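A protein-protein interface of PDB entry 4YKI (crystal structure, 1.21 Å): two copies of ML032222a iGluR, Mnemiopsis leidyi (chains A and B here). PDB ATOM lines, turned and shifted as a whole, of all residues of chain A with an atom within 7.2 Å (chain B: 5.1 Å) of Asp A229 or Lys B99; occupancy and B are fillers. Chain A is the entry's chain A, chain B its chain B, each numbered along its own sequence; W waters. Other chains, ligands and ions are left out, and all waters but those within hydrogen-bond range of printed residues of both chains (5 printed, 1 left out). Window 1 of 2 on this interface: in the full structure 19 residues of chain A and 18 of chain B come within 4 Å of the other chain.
NZ of Lys B99 sits at hydrogen-bond distance from OG of Ser A230, 3.0 Å away.
The side-chain amide oxygen (OD1) of Asn B95 sits at hydrogen-bond distance from the backbone NH (N) of Ala B97, 3.3 Å away. The side-chain carboxylate (OD2) of Asp A229 lies within salt-bridge range of the side-chain amino group (NZ) of Lys A225 (2.7 Å). NZ of Lys B99 is in salt-bridge range of OD1 of Asp B103 (3.99 Å). The backbone carbonyl oxygen of Ser A226 lies within hydrogen-bond range of the side-chain hydroxyl of Ser A230 (3.3 Å). N of Asn B95 sits at hydrogen-bond distance from OH of Tyr B104, 3.1 Å away. The side-chain carboxylate (OD1) of Asp A229 lies within hydrogen-bond range of the backbone NH (N) of Phe A106, at 2.8 Å.
Ser A226 touches Lys B99 (O to NZ, 3.5 Å). CE of Lys B99 touches CB of Asp A229 (3.9 Å). Asn B95 touches Leu A233 (O to CD2, 3.6 Å). Leu A233 touches Lys B99 (CD2 to CB, 3.6 Å). Ser B96 touches Lys A234 (OG to CA, 3.6 Å).
Of the printed residues of chain B, Asp A229 touches Lys B99 (3.9 Å). Printed residues of chain A within 4 Å of Lys B99: Ser A226 (3.5 Å), Asp A229 (3.9 Å), Ser A230 (3.0 Å) and Leu A233 (3.6 Å). Printed residues of chain B within 4 Å of Leu A233: Asn B95 and Lys B99. Of the printed residues of chain A, Asn B95 touches Leu A233. Leu A232 touches none of the printed residues of chain B. Lys A225 touches none of the printed residues of chain B. The nearest printed residue of chain B that does not touch Asp A229 is Tyr B104 (6.1 Å). The nearest printed residue of chain A that does not touch Lys B99 is Leu A227 (5.6 Å).
Along chain A the printed residues that touch a printed residue of chain B span positions 226 to 234. Of the 11 printed residues of chain B, 3 touch a printed residue of chain A. Among the printed residues, 6 pairs touch across the chains.
Position printed for both chains: 104.
Water W3 bridges the side-chain carboxylate (OD1) of Asp B103 (2.7 Å) and the side-chain hydroxyl (OG) of Ser A226 (2.7 Å). Water W4 lies within hydrogen-bond range of the side-chain carboxylate of Asp A229 (2.7 Å) and the side-chain amino group of Lys B99 (3.2 Å). Water W5 bridges the backbone carbonyl oxygen of Ser A230 (2.8 Å) and the side-chain hydroxyl of Ser B96 (2.8 Å). Water W2 lies within hydrogen-bond range of the backbone carbonyl oxygen (O) of Lys B99, the side-chain amino group (NZ) of Lys B220 and the side-chain hydroxyl (OG) of Ser A230. Water W1 lies within hydrogen-bond range of the side-chain carboxylate of Asp A229 (3.0 Å), the side-chain amino group of Lys A225 (3.3 Å) and the backbone carbonyl oxygen of Tyr B104 (3.4 Å).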
ATOM      1  N   LEU A  45     -23.057  -4.815 -15.452  1.00  0.00           N
ATOM      2  CA  LEU A  45     -23.875  -3.750 -16.026  1.00  0.00           C
ATOM      3  C   LEU A  45     -25.318  -4.226 -16.218  1.00  0.00           C
ATOM      4  O   LEU A  45     -26.260  -3.497 -15.918  1.00  0.00           O
ATOM      5  CB  LEU A  45     -23.324  -3.273 -17.371  1.00  0.00           C
ATOM      6  CG  LEU A  45     -22.040  -2.443 -17.362  1.00  0.00           C
ATOM      7  CD1 LEU A  45     -21.463  -2.295 -18.760  1.00  0.00           C
ATOM      8  CD2 LEU A  45     -22.248  -1.068 -16.766  1.00  0.00           C
ATOM      9  N   TYR A 104     -17.239   6.883 -27.987  1.00  0.00           N
ATOM     10  CA  TYR A 104     -16.696   5.971 -27.006  1.00  0.00           C
ATOM     11  C   TYR A 104     -17.340   6.220 -25.658  1.00  0.00           C
ATOM     12  O   TYR A 104     -17.730   7.344 -25.333  1.00  0.00           O
ATOM     13  CB  TYR A 104     -15.194   6.165 -26.876  1.00  0.00           C
ATOM     14  CG  TYR A 104     -14.364   5.687 -28.050  1.00  0.00           C
ATOM     15  CD1 TYR A 104     -14.029   4.353 -28.172  1.00  0.00           C
ATOM     16  CD2 TYR A 104     -13.876   6.573 -29.003  1.00  0.00           C
ATOM     17  CE1 TYR A 104     -13.231   3.907 -29.218  1.00  0.00           C
ATOM     18  CE2 TYR A 104     -13.092   6.135 -30.064  1.00  0.00           C
ATOM     19  CZ  TYR A 104     -12.774   4.800 -30.155  1.00  0.00           C
ATOM     20  OH  TYR A 104     -11.960   4.377 -31.173  1.00  0.00           O
ATOM     21  N   SER A 105     -17.399   5.168 -24.862  1.00  0.00           N
ATOM     22  CA  SER A 105     -17.762   5.291 -23.471  1.00  0.00           C
ATOM     23  C   SER A 105     -16.608   5.912 -22.696  1.00  0.00           C
ATOM     24  O   SER A 105     -15.488   6.042 -23.198  1.00  0.00           O
ATOM     25  CB  SER A 105     -18.056   3.919 -22.862  1.00  0.00           C
ATOM     26  OG  SER A 105     -16.874   3.151 -22.725  1.00  0.00           O
ATOM     27  N   PHE A 106     -16.878   6.220 -21.435  1.00  0.00           N
ATOM     28  CA  PHE A 106     -15.822   6.466 -20.470  1.00  0.00           C
ATOM     29  C   PHE A 106     -14.828   5.311 -20.541  1.00  0.00           C
ATOM     30  O   PHE A 106     -15.241   4.150 -20.623  1.00  0.00           O
ATOM     31  CB  PHE A 106     -16.426   6.564 -19.060  1.00  0.00           C
ATOM     32  CG  PHE A 106     -15.454   7.088 -18.037  1.00  0.00           C
ATOM     33  CD1 PHE A 106     -15.251   8.453 -17.899  1.00  0.00           C
ATOM     34  CD2 PHE A 106     -14.703   6.226 -17.252  1.00  0.00           C
ATOM     35  CE1 PHE A 106     -14.344   8.949 -16.993  1.00  0.00           C
ATOM     36  CE2 PHE A 106     -13.776   6.733 -16.330  1.00  0.00           C
ATOM     37  CZ  PHE A 106     -13.609   8.094 -16.215  1.00  0.00           C
ATOM     38  N   PRO A 107     -13.522   5.610 -20.543  1.00  0.00           N
ATOM     39  CA  PRO A 107     -12.542   4.544 -20.777  1.00  0.00           C
ATOM     40  C   PRO A 107     -12.157   3.810 -19.514  1.00  0.00           C
ATOM     41  O   PRO A 107     -12.322   4.351 -18.418  1.00  0.00           O
ATOM     42  CB  PRO A 107     -11.331   5.300 -21.324  1.00  0.00           C
ATOM     43  CG  PRO A 107     -11.416   6.640 -20.671  1.00  0.00           C
ATOM     44  CD  PRO A 107     -12.879   6.939 -20.548  1.00  0.00           C
ATOM     45  N   PHE A 216     -15.657   1.146 -24.477  1.00  0.00           N
ATOM     46  CA  PHE A 216     -16.701   0.540 -25.303  1.00  0.00           C
ATOM     47  C   PHE A 216     -17.059   1.513 -26.430  1.00  0.00           C
ATOM     48  O   PHE A 216     -16.858   2.725 -26.302  1.00  0.00           O
ATOM     49  CB  PHE A 216     -17.942   0.209 -24.465  1.00  0.00           C
ATOM     50  CG  PHE A 216     -17.768  -0.947 -23.488  1.00  0.00           C
ATOM     51  CD1 PHE A 216     -16.619  -1.738 -23.475  1.00  0.00           C
ATOM     52  CD2 PHE A 216     -18.790  -1.255 -22.585  1.00  0.00           C
ATOM     53  CE1 PHE A 216     -16.497  -2.801 -22.575  1.00  0.00           C
ATOM     54  CE2 PHE A 216     -18.664  -2.320 -21.703  1.00  0.00           C
ATOM     55  CZ  PHE A 216     -17.510  -3.080 -21.698  1.00  0.00           C
ATOM     56  N   LEU A 218     -19.981   3.213 -28.893  1.00  0.00           N
ATOM     57  CA  LEU A 218     -21.390   3.565 -28.880  1.00  0.00           C
ATOM     58  C   LEU A 218     -21.732   4.323 -30.145  1.00  0.00           C
ATOM     59  O   LEU A 218     -20.923   5.136 -30.623  1.00  0.00           O
ATOM     60  CB  LEU A 218     -21.684   4.444 -27.676  1.00  0.00           C
ATOM     61  CG  LEU A 218     -21.635   3.716 -26.346  1.00  0.00           C
ATOM     62  CD1 LEU A 218     -21.410   4.704 -25.220  1.00  0.00           C
ATOM     63  CD2 LEU A 218     -22.919   2.951 -26.157  1.00  0.00           C
ATOM     64  N   TYR A 224     -28.136   5.525 -24.475  1.00  0.00           N
ATOM     65  CA  TYR A 224     -27.599   4.751 -23.368  1.00  0.00           C
ATOM     66  C   TYR A 224     -26.241   5.238 -22.877  1.00  0.00           C
ATOM     67  O   TYR A 224     -25.745   4.738 -21.878  1.00  0.00           O
ATOM     68  CB  TYR A 224     -27.476   3.279 -23.757  1.00  0.00           C
ATOM     69  CG  TYR A 224     -28.752   2.650 -24.271  1.00  0.00           C
ATOM     70  CD1 TYR A 224     -29.954   2.804 -23.591  1.00  0.00           C
ATOM     71  CD2 TYR A 224     -28.752   1.898 -25.440  1.00  0.00           C
ATOM     72  CE1 TYR A 224     -31.116   2.219 -24.055  1.00  0.00           C
ATOM     73  CE2 TYR A 224     -29.917   1.314 -25.919  1.00  0.00           C
ATOM     74  CZ  TYR A 224     -31.094   1.480 -25.218  1.00  0.00           C
ATOM     75  OH  TYR A 224     -32.260   0.904 -25.668  1.00  0.00           O
ATOM     76  N   LYS A 225     -25.643   6.204 -23.567  1.00  0.00           N
ATOM     77  CA  LYS A 225     -24.263   6.596 -23.268  1.00  0.00           C
ATOM     78  C   LYS A 225     -24.070   7.136 -21.857  1.00  0.00           C
ATOM     79  O   LYS A 225     -23.121   6.757 -21.183  1.00  0.00           O
ATOM     80  CB  LYS A 225     -23.723   7.606 -24.278  1.00  0.00           C
ATOM     81  CG  LYS A 225     -22.309   8.103 -23.961  1.00  0.00           C
ATOM     82  CD  LYS A 225     -21.654   8.865 -25.117  1.00  0.00           C
ATOM     83  CE  LYS A 225     -20.501   9.772 -24.646  1.00  0.00           C
ATOM     84  NZ  LYS A 225     -19.419   9.067 -23.914  1.00  0.00           N
ATOM     85  N   SER A 226     -24.951   8.028 -21.407  1.00  0.00           N
ATOM     86  CA  SER A 226     -24.822   8.596 -20.061  1.00  0.00           C
ATOM     87  C   SER A 226     -24.743   7.507 -19.000  1.00  0.00           C
ATOM     88  O   SER A 226     -23.843   7.508 -18.155  1.00  0.00           O
ATOM     89  CB  SER A 226     -25.985   9.549 -19.737  1.00  0.00           C
ATOM     90  OG  SER A 226     -25.949   9.976 -18.374  1.00  0.00           O
ATOM     91  N   LEU A 227     -25.683   6.569 -19.059  1.00  0.00           N
ATOM     92  CA  LEU A 227     -25.772   5.509 -18.050  1.00  0.00           C
ATOM     93  C   LEU A 227     -24.571   4.578 -18.129  1.00  0.00           C
ATOM     94  O   LEU A 227     -24.013   4.201 -17.095  1.00  0.00           O
ATOM     95  CB  LEU A 227     -27.082   4.703 -18.169  1.00  0.00           C
ATOM     96  CG  LEU A 227     -28.329   5.343 -17.568  1.00  0.00           C
ATOM     97  CD1 LEU A 227     -29.564   4.589 -18.006  1.00  0.00           C
ATOM     98  CD2 LEU A 227     -28.213   5.372 -16.051  1.00  0.00           C
ATOM     99  N   ILE A 228     -24.168   4.199 -19.340  1.00  0.00           N
ATOM    100  CA  ILE A 228     -22.994   3.355 -19.455  1.00  0.00           C
ATOM    101  C   ILE A 228     -21.761   4.080 -18.905  1.00  0.00           C
ATOM    102  O   ILE A 228     -20.989   3.506 -18.137  1.00  0.00           O
ATOM    103  CB  ILE A 228     -22.767   2.916 -20.929  1.00  0.00           C
ATOM    104  CG1 ILE A 228     -23.924   2.014 -21.401  1.00  0.00           C
ATOM    105  CG2 ILE A 228     -21.421   2.217 -21.101  1.00  0.00           C
ATOM    106  CD1 ILE A 228     -24.044   0.713 -20.663  1.00  0.00           C
ATOM    107  N   ASP A 229     -21.581   5.343 -19.288  1.00  0.00           N
ATOM    108  CA  ASP A 229     -20.444   6.120 -18.805  1.00  0.00           C
ATOM    109  C   ASP A 229     -20.424   6.187 -17.271  1.00  0.00           C
ATOM    110  O   ASP A 229     -19.396   6.003 -16.639  1.00  0.00           O
ATOM    111  CB  ASP A 229     -20.512   7.552 -19.353  1.00  0.00           C
ATOM    112  CG  ASP A 229     -20.074   7.670 -20.802  1.00  0.00           C
ATOM    113  OD1 ASP A 229     -19.646   6.652 -21.399  1.00  0.00           O
ATOM    114  OD2 ASP A 229     -20.175   8.802 -21.342  1.00  0.00           O
ATOM    115  N   SER A 230     -21.562   6.493 -16.661  1.00  0.00           N
ATOM    116  CA  SER A 230     -21.665   6.599 -15.205  1.00  0.00           C
ATOM    117  C   SER A 230     -21.289   5.302 -14.518  1.00  0.00           C
ATOM    118  O   SER A 230     -20.575   5.284 -13.517  1.00  0.00           O
ATOM    119  CB  SER A 230     -23.094   6.950 -14.791  1.00  0.00           C
ATOM    120  OG  SER A 230     -23.389   8.316 -14.979  1.00  0.00           O
ATOM    121  N   HIS A 231     -21.800   4.196 -15.053  1.00  0.00           N
ATOM    122  CA  HIS A 231     -21.549   2.911 -14.427  1.00  0.00           C
ATOM    123  C   HIS A 231     -20.099   2.445 -14.633  1.00  0.00           C
ATOM    124  O   HIS A 231     -19.515   1.865 -13.721  1.00  0.00           O
ATOM    125  CB  HIS A 231     -22.608   1.882 -14.852  1.00  0.00           C
ATOM    126  CG  HIS A 231     -23.910   2.051 -14.120  1.00  0.00           C
ATOM    127  ND1 HIS A 231     -24.395   1.132 -13.213  1.00  0.00           N
ATOM    128  CD2 HIS A 231     -24.858   3.011 -14.215  1.00  0.00           C
ATOM    129  CE1 HIS A 231     -25.574   1.531 -12.768  1.00  0.00           C
ATOM    130  NE2 HIS A 231     -25.872   2.673 -13.351  1.00  0.00           N
ATOM    131  N   LEU A 232     -19.499   2.715 -15.796  1.00  0.00           N
ATOM    132  CA  LEU A 232     -18.085   2.392 -15.987  1.00  0.00           C
ATOM    133  C   LEU A 232     -17.173   3.216 -15.070  1.00  0.00           C
ATOM    134  O   LEU A 232     -16.197   2.696 -14.557  1.00  0.00           O
ATOM    135  CB  LEU A 232     -17.667   2.538 -17.444  1.00  0.00           C
ATOM    136  CG  LEU A 232     -18.254   1.494 -18.403  1.00  0.00           C
ATOM    137  CD1 LEU A 232     -17.839   1.841 -19.822  1.00  0.00           C
ATOM    138  CD2 LEU A 232     -17.850   0.075 -18.025  1.00  0.00           C
ATOM    139  N   LEU A 233     -17.487   4.487 -14.857  1.00  0.00           N
ATOM    140  CA  LEU A 233     -16.701   5.289 -13.922  1.00  0.00           C
ATOM    141  C   LEU A 233     -16.824   4.720 -12.514  1.00  0.00           C
ATOM    142  O   LEU A 233     -15.830   4.590 -11.812  1.00  0.00           O
ATOM    143  CB  LEU A 233     -17.134   6.755 -13.974  1.00  0.00           C
ATOM    144  CG  LEU A 233     -16.603   7.654 -12.850  1.00  0.00           C
ATOM    145  CD1 LEU A 233     -15.112   7.663 -12.833  1.00  0.00           C
ATOM    146  CD2 LEU A 233     -17.114   9.072 -13.017  1.00  0.00           C
ATOM    147  N   LYS A 234     -18.039   4.357 -12.121  1.00  0.00           N
ATOM    148  CA  LYS A 234     -18.249   3.754 -10.816  1.00  0.00           C
ATOM    149  C   LYS A 234     -17.438   2.456 -10.679  1.00  0.00           C
ATOM    150  O   LYS A 234     -16.831   2.221  -9.654  1.00  0.00           O
ATOM    151  CB  LYS A 234     -19.744   3.505 -10.590  1.00  0.00           C
ATOM    152  CG  LYS A 234     -20.080   2.847  -9.283  1.00  0.00           C
ATOM    153  CD  LYS A 234     -21.602   2.820  -9.097  1.00  0.00           C
ATOM    154  CE  LYS A 234     -22.025   2.151  -7.799  1.00  0.00           C
ATOM    155  NZ  LYS A 234     -23.481   2.323  -7.545  1.00  0.00           N
ATOM    156  N   PHE A 235     -17.419   1.612 -11.714  1.00  0.00           N
ATOM    157  CA  PHE A 235     -16.600   0.395 -11.667  1.00  0.00           C
ATOM    158  C   PHE A 235     -15.129   0.739 -11.391  1.00  0.00           C
ATOM    159  O   PHE A 235     -14.444   0.080 -10.615  1.00  0.00           O
ATOM    160  CB  PHE A 235     -16.615  -0.341 -13.013  1.00  0.00           C
ATOM    161  CG  PHE A 235     -17.883  -1.107 -13.333  1.00  0.00           C
ATOM    162  CD1 PHE A 235     -18.947  -1.206 -12.456  1.00  0.00           C
ATOM    163  CD2 PHE A 235     -17.983  -1.751 -14.552  1.00  0.00           C
ATOM    164  CE1 PHE A 235     -20.080  -1.936 -12.801  1.00  0.00           C
ATOM    165  CE2 PHE A 235     -19.116  -2.482 -14.893  1.00  0.00           C
ATOM    166  CZ  PHE A 235     -20.158  -2.557 -14.024  1.00  0.00           C
ATOM    167  N   ASN B  95     -14.899  11.620 -10.537  1.00  0.00           N
ATOM    168  CA  ASN B  95     -15.519  10.854  -9.452  1.00  0.00           C
ATOM    169  C   ASN B  95     -17.018  10.731  -9.660  1.00  0.00           C
ATOM    170  O   ASN B  95     -17.632  11.507 -10.382  1.00  0.00           O
ATOM    171  CB  ASN B  95     -15.126  11.346  -8.036  1.00  0.00           C
ATOM    172  CG  ASN B  95     -15.653  12.721  -7.681  1.00  0.00           C
ATOM    173  OD1 ASN B  95     -16.849  12.969  -7.733  1.00  0.00           O
ATOM    174  ND2 ASN B  95     -14.758  13.591  -7.220  1.00  0.00           N
ATOM    175  N   SER B  96     -17.587   9.709  -9.046  1.00  0.00           N
ATOM    176  CA  SER B  96     -18.988   9.384  -9.242  1.00  0.00           C
ATOM    177  C   SER B  96     -19.920  10.482  -8.712  1.00  0.00           C
ATOM    178  O   SER B  96     -20.971  10.740  -9.287  1.00  0.00           O
ATOM    179  CB  SER B  96     -19.313   8.032  -8.612  1.00  0.00           C
ATOM    180  OG  SER B  96     -18.688   6.972  -9.327  1.00  0.00           O
ATOM    181  N   ALA B  97     -19.552  11.122  -7.608  1.00  0.00           N
ATOM    182  CA  ALA B  97     -20.381  12.190  -7.063  1.00  0.00           C
ATOM    183  C   ALA B  97     -20.544  13.299  -8.123  1.00  0.00           C
ATOM    184  O   ALA B  97     -21.648  13.724  -8.422  1.00  0.00           O
ATOM    185  CB  ALA B  97     -19.787  12.751  -5.759  1.00  0.00           C
ATOM    186  N   ARG B  98     -19.431  13.745  -8.708  1.00  0.00           N
ATOM    187  CA  ARG B  98     -19.461  14.771  -9.740  1.00  0.00           C
ATOM    188  C   ARG B  98     -20.254  14.293 -10.969  1.00  0.00           C
ATOM    189  O   ARG B  98     -21.022  15.047 -11.533  1.00  0.00           O
ATOM    190  CB  ARG B  98     -18.028  15.183 -10.127  1.00  0.00           C
ATOM    191  CG  ARG B  98     -17.377  16.074  -9.091  1.00  0.00           C
ATOM    192  CD  ARG B  98     -15.895  16.240  -9.339  1.00  0.00           C
ATOM    193  NE  ARG B  98     -15.311  17.144  -8.366  1.00  0.00           N
ATOM    194  CZ  ARG B  98     -14.020  17.403  -8.285  1.00  0.00           C
ATOM    195  NH1 ARG B  98     -13.151  16.843  -9.111  1.00  0.00           N
ATOM    196  NH2 ARG B  98     -13.591  18.272  -7.384  1.00  0.00           N
ATOM    197  N   LYS B  99     -20.050  13.035 -11.359  1.00  0.00           N
ATOM    198  CA  LYS B  99     -20.712  12.446 -12.516  1.00  0.00           C
ATOM    199  C   LYS B  99     -22.229  12.423 -12.350  1.00  0.00           C
ATOM    200  O   LYS B  99     -22.953  12.410 -13.335  1.00  0.00           O
ATOM    201  CB  LYS B  99     -20.163  11.038 -12.768  1.00  0.00           C
ATOM    202  CG  LYS B  99     -20.646  10.338 -14.045  1.00  0.00           C
ATOM    203  CD  LYS B  99     -20.233  11.075 -15.318  1.00  0.00           C
ATOM    204  CE  LYS B  99     -20.605  10.305 -16.589  1.00  0.00           C
ATOM    205  NZ  LYS B  99     -22.079  10.255 -16.820  1.00  0.00           N
ATOM    206  N   SER B 100     -22.725  12.428 -11.116  1.00  0.00           N
ATOM    207  CA  SER B 100     -24.177  12.478 -10.906  1.00  0.00           C
ATOM    208  C   SER B 100     -24.781  13.848 -11.257  1.00  0.00           C
ATOM    209  O   SER B 100     -25.991  13.947 -11.452  1.00  0.00           O
ATOM    210  CB  SER B 100     -24.529  12.084  -9.464  1.00  0.00           C
ATOM    211  OG  SER B 100     -24.275  13.148  -8.569  1.00  0.00           O
ATOM    212  N   ALA B 101     -23.932  14.875 -11.365  1.00  0.00           N
ATOM    213  CA  ALA B 101     -24.357  16.256 -11.598  1.00  0.00           C
ATOM    214  C   ALA B 101     -23.885  16.838 -12.917  1.00  0.00           C
ATOM    215  O   ALA B 101     -24.584  17.676 -13.480  1.00  0.00           O
ATOM    216  CB  ALA B 101     -23.888  17.150 -10.452  1.00  0.00           C
ATOM    217  N   ILE B 102     -22.684  16.453 -13.364  1.00  0.00           N
ATOM    218  CA  ILE B 102     -22.077  17.000 -14.583  1.00  0.00           C
ATOM    219  C   ILE B 102     -21.521  15.868 -15.437  1.00  0.00           C
ATOM    220  O   ILE B 102     -21.467  14.720 -14.995  1.00  0.00           O
ATOM    221  CB  ILE B 102     -20.920  18.007 -14.255  1.00  0.00           C
ATOM    222  CG1 ILE B 102     -19.712  17.325 -13.595  1.00  0.00           C
ATOM    223  CG2 ILE B 102     -21.451  19.166 -13.394  1.00  0.00           C
ATOM    224  CD1 ILE B 102     -18.399  18.110 -13.757  1.00  0.00           C
ATOM    225  N   ASP B 103     -21.114  16.205 -16.654  1.00  0.00           N
ATOM    226  CA  ASP B 103     -20.386  15.290 -17.521  1.00  0.00           C
ATOM    227  C   ASP B 103     -18.904  15.622 -17.492  1.00  0.00           C
ATOM    228  O   ASP B 103     -18.477  16.695 -17.028  1.00  0.00           O
ATOM    229  CB  ASP B 103     -20.891  15.385 -18.960  1.00  0.00           C
ATOM    230  CG  ASP B 103     -22.225  14.667 -19.184  1.00  0.00           C
ATOM    231  OD1 ASP B 103     -22.694  13.908 -18.310  1.00  0.00           O
ATOM    232  OD2 ASP B 103     -22.776  14.857 -20.281  1.00  0.00           O
ATOM    233  N   TYR B 104     -18.119  14.680 -17.996  1.00  0.00           N
ATOM    234  CA  TYR B 104     -16.700  14.880 -18.230  1.00  0.00           C
ATOM    235  C   TYR B 104     -16.409  14.768 -19.717  1.00  0.00           C
ATOM    236  O   TYR B 104     -17.063  14.010 -20.434  1.00  0.00           O
ATOM    237  CB  TYR B 104     -15.879  13.841 -17.492  1.00  0.00           C
ATOM    238  CG  TYR B 104     -15.843  14.012 -16.004  1.00  0.00           C
ATOM    239  CD1 TYR B 104     -14.948  14.896 -15.417  1.00  0.00           C
ATOM    240  CD2 TYR B 104     -16.681  13.276 -15.169  1.00  0.00           C
ATOM    241  CE1 TYR B 104     -14.877  15.027 -14.053  1.00  0.00           C
ATOM    242  CE2 TYR B 104     -16.612  13.388 -13.796  1.00  0.00           C
ATOM    243  CZ  TYR B 104     -15.719  14.288 -13.249  1.00  0.00           C
ATOM    244  OH  TYR B 104     -15.627  14.351 -11.892  1.00  0.00           O
ATOM    245  N   LYS B 220     -24.341  18.747 -18.278  1.00  0.00           N
ATOM    246  CA  LYS B 220     -25.173  17.788 -18.974  1.00  0.00           C
ATOM    247  C   LYS B 220     -25.894  18.529 -20.094  1.00  0.00           C
ATOM    248  O   LYS B 220     -26.278  19.703 -19.961  1.00  0.00           O
ATOM    249  CB  LYS B 220     -26.152  17.117 -18.010  1.00  0.00           C
ATOM    250  CG  LYS B 220     -25.451  16.178 -17.036  1.00  0.00           C
ATOM    251  CD  LYS B 220     -26.441  15.507 -16.104  1.00  0.00           C
ATOM    252  CE  LYS B 220     -25.773  14.450 -15.249  1.00  0.00           C
ATOM    253  NZ  LYS B 220     -26.740  13.540 -14.591  1.00  0.00           N
HETATM  254  O   HOH W   1     -18.017  10.936 -21.538  1.00  0.00           O
HETATM  255  O   HOH W   2     -25.037  10.950 -14.594  1.00  0.00           O
HETATM  256  O   HOH W   3     -25.008  12.539 -18.462  1.00  0.00           O
HETATM  257  O   HOH W   4     -21.526  10.710 -19.943  1.00  0.00           O
HETATM  258  O   HOH W   5     -20.201   7.369 -11.690  1.00  0.00           O
